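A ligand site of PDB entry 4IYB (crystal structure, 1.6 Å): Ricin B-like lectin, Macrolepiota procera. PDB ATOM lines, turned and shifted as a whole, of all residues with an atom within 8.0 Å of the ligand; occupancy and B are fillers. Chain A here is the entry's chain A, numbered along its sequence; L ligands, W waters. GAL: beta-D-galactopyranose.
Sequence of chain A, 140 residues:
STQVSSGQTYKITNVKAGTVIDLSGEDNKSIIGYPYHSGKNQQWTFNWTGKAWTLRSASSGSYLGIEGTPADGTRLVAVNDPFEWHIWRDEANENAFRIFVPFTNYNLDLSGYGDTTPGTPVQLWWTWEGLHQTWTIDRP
An oxygen (O4) of the ligand lies within hydrogen-bond range of the side-chain carboxylate (OD1) of Asp 22, at 2.6 Å. N of Gly 25 sits at hydrogen-bond distance from O4 of the ligand (2.8 Å). A ring nitrogen (NE2) of His 37 sits at hydrogen-bond distance from an oxygen (O3) of the ligand, 2.8 Å away. O3 of the ligand sits at hydrogen-bond distance from ND2 of Asn 41, at 3.0 Å. The side-chain carboxylate of Glu 26 sits close to an oxygen (O6) of the ligand (3.5 Å).
ND2 of Asn 41 lies within hydrogen-bond range of OD1 of Asp 22, at 3.3 Å. The side-chain carboxylate (OD1) of Asp 22 is in hydrogen-bond range of the backbone NH (N) of Ser 24, 3.5 Å away. The backbone NH of Asp 22 sits at hydrogen-bond distance from the backbone carbonyl oxygen of Ile 32 (2.9 Å). N of His 37 sits at hydrogen-bond distance from OE1 of Gln 42 (2.8 Å). O of Asn 41 sits at hydrogen-bond distance from N of Leu 23. The side-chain hydroxyl (OG) of Ser 24 sits at hydrogen-bond distance from the backbone NH (N) of Glu 26, 3.0 Å away. O of Tyr 34 is in hydrogen-bond range of N of Val 20, 2.9 Å away. The side-chain amide oxygen of Gln 42 sits at hydrogen-bond distance from the backbone NH of Gly 39, 3.1 Å away.
Leu 23 touches the ligand (O to O4, 3.7 Å). CA of Ser 24 touches O4 of the ligand, 3.3 Å away. Ile 32 touches the ligand (CD1 to C6, 3.8 Å). Tyr 34 touches the ligand (CE2 to C5, 3.7 Å). Gln 42 touches the ligand (NE2 to O3, 3.7 Å). Hydrophobic or aromatic side chains within 4 Å of the ligand: Ile 32, Tyr 34 and His 37.
Water W2 lies within hydrogen-bond range of the side-chain amide oxygen (OD1) of Asn 41 (2.6 Å) and an oxygen (O2) of the ligand (2.8 Å).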
ATOM      1  N   VAL A  20      -8.723   2.162  13.680  1.00  0.00           N
ATOM      2  CA  VAL A  20      -9.827   1.813  14.567  1.00  0.00           C
ATOM      3  C   VAL A  20     -10.074   0.332  14.654  1.00  0.00           C
ATOM      4  O   VAL A  20      -9.640  -0.451  13.811  1.00  0.00           O
ATOM      5  CB  VAL A  20     -11.141   2.517  14.174  1.00  0.00           C
ATOM      6  CG1 VAL A  20     -10.965   4.012  14.117  1.00  0.00           C
ATOM      7  CG2 VAL A  20     -11.696   1.935  12.876  1.00  0.00           C
ATOM      8  N   ILE A  21     -10.746  -0.080  15.726  1.00  0.00           N
ATOM      9  CA  ILE A  21     -11.180  -1.445  15.890  1.00  0.00           C
ATOM     10  C   ILE A  21     -12.270  -1.769  14.877  1.00  0.00           C
ATOM     11  O   ILE A  21     -13.330  -1.167  14.883  1.00  0.00           O
ATOM     12  CB  ILE A  21     -11.694  -1.678  17.327  1.00  0.00           C
ATOM     13  CG1 ILE A  21     -10.574  -1.347  18.335  1.00  0.00           C
ATOM     14  CG2 ILE A  21     -12.188  -3.099  17.503  1.00  0.00           C
ATOM     15  CD1 ILE A  21     -10.916  -1.716  19.754  1.00  0.00           C
ATOM     16  N   ASP A  22     -11.978  -2.759  14.046  1.00  0.00           N
ATOM     17  CA  ASP A  22     -12.717  -3.036  12.806  1.00  0.00           C
ATOM     18  C   ASP A  22     -13.017  -4.534  12.765  1.00  0.00           C
ATOM     19  O   ASP A  22     -12.142  -5.355  12.988  1.00  0.00           O
ATOM     20  CB  ASP A  22     -11.830  -2.562  11.654  1.00  0.00           C
ATOM     21  CG  ASP A  22     -12.410  -2.844  10.248  1.00  0.00           C
ATOM     22  OD1 ASP A  22     -12.700  -4.016   9.943  1.00  0.00           O
ATOM     23  OD2 ASP A  22     -12.452  -1.863   9.446  1.00  0.00           O
ATOM     24  N   LEU A  23     -14.293  -4.867  12.579  1.00  0.00           N
ATOM     25  CA  LEU A  23     -14.704  -6.242  12.317  1.00  0.00           C
ATOM     26  C   LEU A  23     -14.477  -6.534  10.818  1.00  0.00           C
ATOM     27  O   LEU A  23     -15.157  -5.984   9.957  1.00  0.00           O
ATOM     28  CB  LEU A  23     -16.176  -6.397  12.684  1.00  0.00           C
ATOM     29  CG  LEU A  23     -16.794  -7.778  12.386  1.00  0.00           C
ATOM     30  CD1 LEU A  23     -16.062  -8.850  13.148  1.00  0.00           C
ATOM     31  CD2 LEU A  23     -18.292  -7.799  12.675  1.00  0.00           C
ATOM     32  N   SER A  24     -13.469  -7.329  10.544  1.00  0.00           N
ATOM     33  CA  SER A  24     -12.989  -7.561   9.186  1.00  0.00           C
ATOM     34  C   SER A  24     -14.086  -7.910   8.211  1.00  0.00           C
ATOM     35  O   SER A  24     -14.848  -8.846   8.412  1.00  0.00           O
ATOM     36  CB  SER A  24     -11.992  -8.688   9.190  1.00  0.00           C
ATOM     37  OG  SER A  24     -11.592  -8.956   7.857  1.00  0.00           O
ATOM     38  N   GLY A  25     -14.080  -7.192   7.098  1.00  0.00           N
ATOM     39  CA  GLY A  25     -15.004  -7.489   6.016  1.00  0.00           C
ATOM     40  C   GLY A  25     -14.605  -8.736   5.253  1.00  0.00           C
ATOM     41  O   GLY A  25     -15.395  -9.216   4.450  1.00  0.00           O
ATOM     42  N   GLU A  26     -13.430  -9.282   5.500  1.00  0.00           N
ATOM     43  CA  GLU A  26     -13.016 -10.529   4.840  1.00  0.00           C
ATOM     44  C   GLU A  26     -13.714 -11.745   5.402  1.00  0.00           C
ATOM     45  O   GLU A  26     -14.007 -12.683   4.667  1.00  0.00           O
ATOM     46  CB  GLU A  26     -11.515 -10.699   4.956  1.00  0.00           C
ATOM     47  CG  GLU A  26     -10.767  -9.599   4.217  1.00  0.00           C
ATOM     48  CD  GLU A  26      -9.294  -9.875   4.037  1.00  0.00           C
ATOM     49  OE1 GLU A  26      -8.659  -9.201   3.206  1.00  0.00           O
ATOM     50  OE2 GLU A  26      -8.774 -10.769   4.747  1.00  0.00           O
ATOM     51  N   ASP A  27     -13.990 -11.745   6.704  1.00  0.00           N
ATOM     52  CA  ASP A  27     -14.527 -12.942   7.365  1.00  0.00           C
ATOM     53  C   ASP A  27     -15.644 -12.705   8.359  1.00  0.00           C
ATOM     54  O   ASP A  27     -16.228 -13.666   8.882  1.00  0.00           O
ATOM     55  CB  ASP A  27     -13.416 -13.817   7.950  1.00  0.00           C
ATOM     56  CG  ASP A  27     -12.663 -13.130   9.097  1.00  0.00           C
ATOM     57  OD1 ASP A  27     -13.141 -12.077   9.582  1.00  0.00           O
ATOM     58  OD2 ASP A  27     -11.639 -13.673   9.498  1.00  0.00           O
ATOM     59  N   ASN A  28     -15.971 -11.431   8.592  1.00  0.00           N
ATOM     60  CA  ASN A  28     -16.923 -11.000   9.616  1.00  0.00           C
ATOM     61  C   ASN A  28     -16.658 -11.633  10.984  1.00  0.00           C
ATOM     62  O   ASN A  28     -17.588 -11.840  11.746  1.00  0.00           O
ATOM     63  CB  ASN A  28     -18.386 -11.259   9.160  1.00  0.00           C
ATOM     64  CG  ASN A  28     -18.770 -10.470   7.914  1.00  0.00           C
ATOM     65  OD1 ASN A  28     -18.376  -9.320   7.728  1.00  0.00           O
ATOM     66  ND2 ASN A  28     -19.501 -11.115   7.009  1.00  0.00           N
ATOM     67  N   SER A  30     -12.757 -11.706  12.409  1.00  0.00           N
ATOM     68  CA  SER A  30     -11.466 -11.249  12.916  1.00  0.00           C
ATOM     69  C   SER A  30     -11.529  -9.760  13.244  1.00  0.00           C
ATOM     70  O   SER A  30     -12.147  -8.991  12.530  1.00  0.00           O
ATOM     71  CB  SER A  30     -10.414 -11.464  11.854  1.00  0.00           C
ATOM     72  OG  SER A  30     -10.279 -12.855  11.546  1.00  0.00           O
ATOM     73  N   ILE A  32      -9.449  -6.328  13.724  1.00  0.00           N
ATOM     74  CA  ILE A  32      -8.243  -5.763  13.146  1.00  0.00           C
ATOM     75  C   ILE A  32      -8.234  -4.238  13.334  1.00  0.00           C
ATOM     76  O   ILE A  32      -9.271  -3.615  13.618  1.00  0.00           O
ATOM     77  CB  ILE A  32      -8.173  -6.063  11.611  1.00  0.00           C
ATOM     78  CG1 ILE A  32      -9.354  -5.458  10.876  1.00  0.00           C
ATOM     79  CG2 ILE A  32      -8.001  -7.553  11.373  1.00  0.00           C
ATOM     80  CD1 ILE A  32      -9.349  -5.736   9.400  1.00  0.00           C
ATOM     81  N   GLY A  33      -7.040  -3.659  13.248  1.00  0.00           N
ATOM     82  CA  GLY A  33      -6.877  -2.221  13.133  1.00  0.00           C
ATOM     83  C   GLY A  33      -6.988  -1.825  11.668  1.00  0.00           C
ATOM     84  O   GLY A  33      -6.264  -2.359  10.819  1.00  0.00           O
ATOM     85  N   TYR A  34      -7.870  -0.887  11.387  1.00  0.00           N
ATOM     86  CA  TYR A  34      -8.106  -0.438  10.000  1.00  0.00           C
ATOM     87  C   TYR A  34      -8.414   1.047   9.978  1.00  0.00           C
ATOM     88  O   TYR A  34      -9.086   1.564  10.871  1.00  0.00           O
ATOM     89  CB  TYR A  34      -9.287  -1.237   9.377  1.00  0.00           C
ATOM     90  CG  TYR A  34      -9.206  -1.418   7.864  1.00  0.00           C
ATOM     91  CD1 TYR A  34      -9.759  -0.470   6.995  1.00  0.00           C
ATOM     92  CD2 TYR A  34      -8.499  -2.494   7.303  1.00  0.00           C
ATOM     93  CE1 TYR A  34      -9.623  -0.612   5.620  1.00  0.00           C
ATOM     94  CE2 TYR A  34      -8.399  -2.632   5.938  1.00  0.00           C
ATOM     95  CZ  TYR A  34      -8.940  -1.690   5.118  1.00  0.00           C
ATOM     96  OH  TYR A  34      -8.749  -1.846   3.738  1.00  0.00           O
ATOM     97  N   PRO A  35      -7.975   1.763   8.932  1.00  0.00           N
ATOM     98  CA  PRO A  35      -8.343   3.168   8.855  1.00  0.00           C
ATOM     99  C   PRO A  35      -9.844   3.375   8.856  1.00  0.00           C
ATOM    100  O   PRO A  35     -10.590   2.637   8.182  1.00  0.00           O
ATOM    101  CB  PRO A  35      -7.730   3.596   7.496  1.00  0.00           C
ATOM    102  CG  PRO A  35      -6.558   2.692   7.315  1.00  0.00           C
ATOM    103  CD  PRO A  35      -7.014   1.379   7.879  1.00  0.00           C
ATOM    104  N   TYR A  36     -10.306   4.395   9.582  1.00  0.00           N
ATOM    105  CA  TYR A  36     -11.740   4.660   9.687  1.00  0.00           C
ATOM    106  C   TYR A  36     -12.290   5.181   8.361  1.00  0.00           C
ATOM    107  O   TYR A  36     -11.700   6.112   7.775  1.00  0.00           O
ATOM    108  CB  TYR A  36     -12.002   5.707  10.773  1.00  0.00           C
ATOM    109  CG  TYR A  36     -13.471   5.840  11.120  1.00  0.00           C
ATOM    110  CD1 TYR A  36     -14.220   4.773  11.595  1.00  0.00           C
ATOM    111  CD2 TYR A  36     -14.127   7.058  10.933  1.00  0.00           C
ATOM    112  CE1 TYR A  36     -15.551   4.915  11.932  1.00  0.00           C
ATOM    113  CE2 TYR A  36     -15.458   7.200  11.269  1.00  0.00           C
ATOM    114  CZ  TYR A  36     -16.176   6.110  11.757  1.00  0.00           C
ATOM    115  OH  TYR A  36     -17.522   6.196  12.093  1.00  0.00           O
ATOM    116  N   HIS A  37     -13.423   4.628   7.952  1.00  0.00           N
ATOM    117  CA  HIS A  37     -14.137   5.112   6.747  1.00  0.00           C
ATOM    118  C   HIS A  37     -15.634   5.123   6.993  1.00  0.00           C
ATOM    119  O   HIS A  37     -16.435   5.024   6.057  1.00  0.00           O
ATOM    120  CB  HIS A  37     -13.818   4.242   5.542  1.00  0.00           C
ATOM    121  CG  HIS A  37     -14.151   2.801   5.724  1.00  0.00           C
ATOM    122  ND1 HIS A  37     -15.408   2.278   5.452  1.00  0.00           N
ATOM    123  CD2 HIS A  37     -13.393   1.745   6.103  1.00  0.00           C
ATOM    124  CE1 HIS A  37     -15.414   0.985   5.720  1.00  0.00           C
ATOM    125  NE2 HIS A  37     -14.201   0.632   6.107  1.00  0.00           N
ATOM    126  N   SER A  38     -16.024   5.249   8.260  1.00  0.00           N
ATOM    127  CA  SER A  38     -17.448   5.282   8.664  1.00  0.00           C
ATOM    128  C   SER A  38     -18.195   3.987   8.356  1.00  0.00           C
ATOM    129  O   SER A  38     -19.416   4.019   8.114  1.00  0.00           O
ATOM    130  CB  SER A  38     -18.165   6.509   8.054  1.00  0.00           C
ATOM    131  OG  SER A  38     -17.555   7.727   8.426  1.00  0.00           O
ATOM    132  N   GLY A  39     -17.505   2.852   8.318  1.00  0.00           N
ATOM    133  CA  GLY A  39     -18.130   1.562   8.142  1.00  0.00           C
ATOM    134  C   GLY A  39     -18.926   1.150   9.370  1.00  0.00           C
ATOM    135  O   GLY A  39     -18.518   1.421  10.509  1.00  0.00           O
ATOM    136  N   LYS A  40     -20.067   0.491   9.187  1.00  0.00           N
ATOM    137  CA  LYS A  40     -20.826   0.014  10.347  1.00  0.00           C
ATOM    138  C   LYS A  40     -20.056  -1.061  11.074  1.00  0.00           C
ATOM    139  O   LYS A  40     -20.267  -1.279  12.271  1.00  0.00           O
ATOM    140  CB  LYS A  40     -22.212  -0.517   9.922  1.00  0.00           C
ATOM    141  CG  LYS A  40     -23.128   0.574   9.412  1.00  0.00           C
ATOM    142  CD  LYS A  40     -23.442   1.575  10.516  1.00  0.00           C
ATOM    143  CE  LYS A  40     -24.945   1.713  10.722  1.00  0.00           C
ATOM    144  NZ  LYS A  40     -25.510   2.837   9.934  1.00  0.00           N
ATOM    145  N   ASN A  41     -19.179  -1.754  10.372  1.00  0.00           N
ATOM    146  CA  ASN A  41     -18.297  -2.717  10.958  1.00  0.00           C
ATOM    147  C   ASN A  41     -17.143  -2.069  11.753  1.00  0.00           C
ATOM    148  O   ASN A  41     -16.329  -2.786  12.324  1.00  0.00           O
ATOM    149  CB  ASN A  41     -17.703  -3.616   9.877  1.00  0.00           C
ATOM    150  CG  ASN A  41     -16.829  -2.849   8.888  1.00  0.00           C
ATOM    151  OD1 ASN A  41     -17.214  -1.799   8.383  1.00  0.00           O
ATOM    152  ND2 ASN A  41     -15.636  -3.381   8.637  1.00  0.00           N
ATOM    153  N   GLN A  42     -17.120  -0.743  11.768  1.00  0.00           N
ATOM    154  CA  GLN A  42     -16.110   0.023  12.532  1.00  0.00           C
ATOM    155  C   GLN A  42     -16.771   0.761  13.700  1.00  0.00           C
ATOM    156  O   GLN A  42     -16.191   1.686  14.270  1.00  0.00           O
ATOM    157  CB  GLN A  42     -15.419   1.013  11.605  1.00  0.00           C
ATOM    158  CG  GLN A  42     -14.864   0.351  10.348  1.00  0.00           C
ATOM    159  CD  GLN A  42     -14.068   1.321   9.533  1.00  0.00           C
ATOM    160  OE1 GLN A  42     -14.529   2.404   9.197  1.00  0.00           O
ATOM    161  NE2 GLN A  42     -12.819   0.967   9.291  1.00  0.00           N
ATOM    162  N   PRO A 118      -3.033  -1.537   7.675  1.00  0.00           N
ATOM    163  CA  PRO A 118      -4.394  -2.057   7.708  1.00  0.00           C
ATOM    164  C   PRO A 118      -4.442  -3.583   7.825  1.00  0.00           C
ATOM    165  O   PRO A 118      -3.698  -4.302   7.119  1.00  0.00           O
ATOM    166  CB  PRO A 118      -5.007  -1.568   6.392  1.00  0.00           C
ATOM    167  CG  PRO A 118      -4.200  -0.356   6.038  1.00  0.00           C
ATOM    168  CD  PRO A 118      -2.787  -0.687   6.497  1.00  0.00           C
ATOM    169  N   GLY A 119      -5.270  -4.093   8.728  1.00  0.00           N
ATOM    170  CA  GLY A 119      -5.367  -5.521   8.964  1.00  0.00           C
ATOM    171  C   GLY A 119      -4.581  -6.051  10.158  1.00  0.00           C
ATOM    172  O   GLY A 119      -4.624  -7.249  10.475  1.00  0.00           O
HETATM  173  C1  GAL L   1     -13.410  -4.195   4.105  1.00  0.00           C
HETATM  174  C2  GAL L   1     -14.029  -3.321   5.179  1.00  0.00           C
HETATM  175  C3  GAL L   1     -12.934  -2.747   6.055  1.00  0.00           C
HETATM  176  C4  GAL L   1     -12.051  -3.863   6.570  1.00  0.00           C
HETATM  177  C5  GAL L   1     -11.510  -4.639   5.382  1.00  0.00           C
HETATM  178  C6  GAL L   1     -10.636  -5.794   5.815  1.00  0.00           C
HETATM  179  O1  GAL L   1     -14.487  -4.817   3.420  1.00  0.00           O
HETATM  180  O2  GAL L   1     -14.759  -2.258   4.598  1.00  0.00           O
HETATM  181  O3  GAL L   1     -13.545  -1.943   7.043  1.00  0.00           O
HETATM  182  O4  GAL L   1     -12.784  -4.725   7.458  1.00  0.00           O
HETATM  183  O5  GAL L   1     -12.621  -5.198   4.707  1.00  0.00           O
HETATM  184  O6  GAL L   1      -9.945  -6.319   4.705  1.00  0.00           O
HETATM  185  O   HOH W   1     -13.390  -5.630   1.058  1.00  0.00           O
HETATM  186  O   HOH W   2     -17.211  -1.467   5.765  1.00  0.00           O
HETATM  187  O   HOH W   3      -7.115  -6.016   5.702  1.00  0.00           O
HETATM  188  O   HOH W   4     -17.046  -5.000   4.018  1.00  0.00           O
HETATM  189  O   HOH W   5     -10.560  -6.008   1.924  1.00  0.00           O
HETATM  190  O   HOH W   6     -14.222  -0.789   2.693  1.00  0.00           O
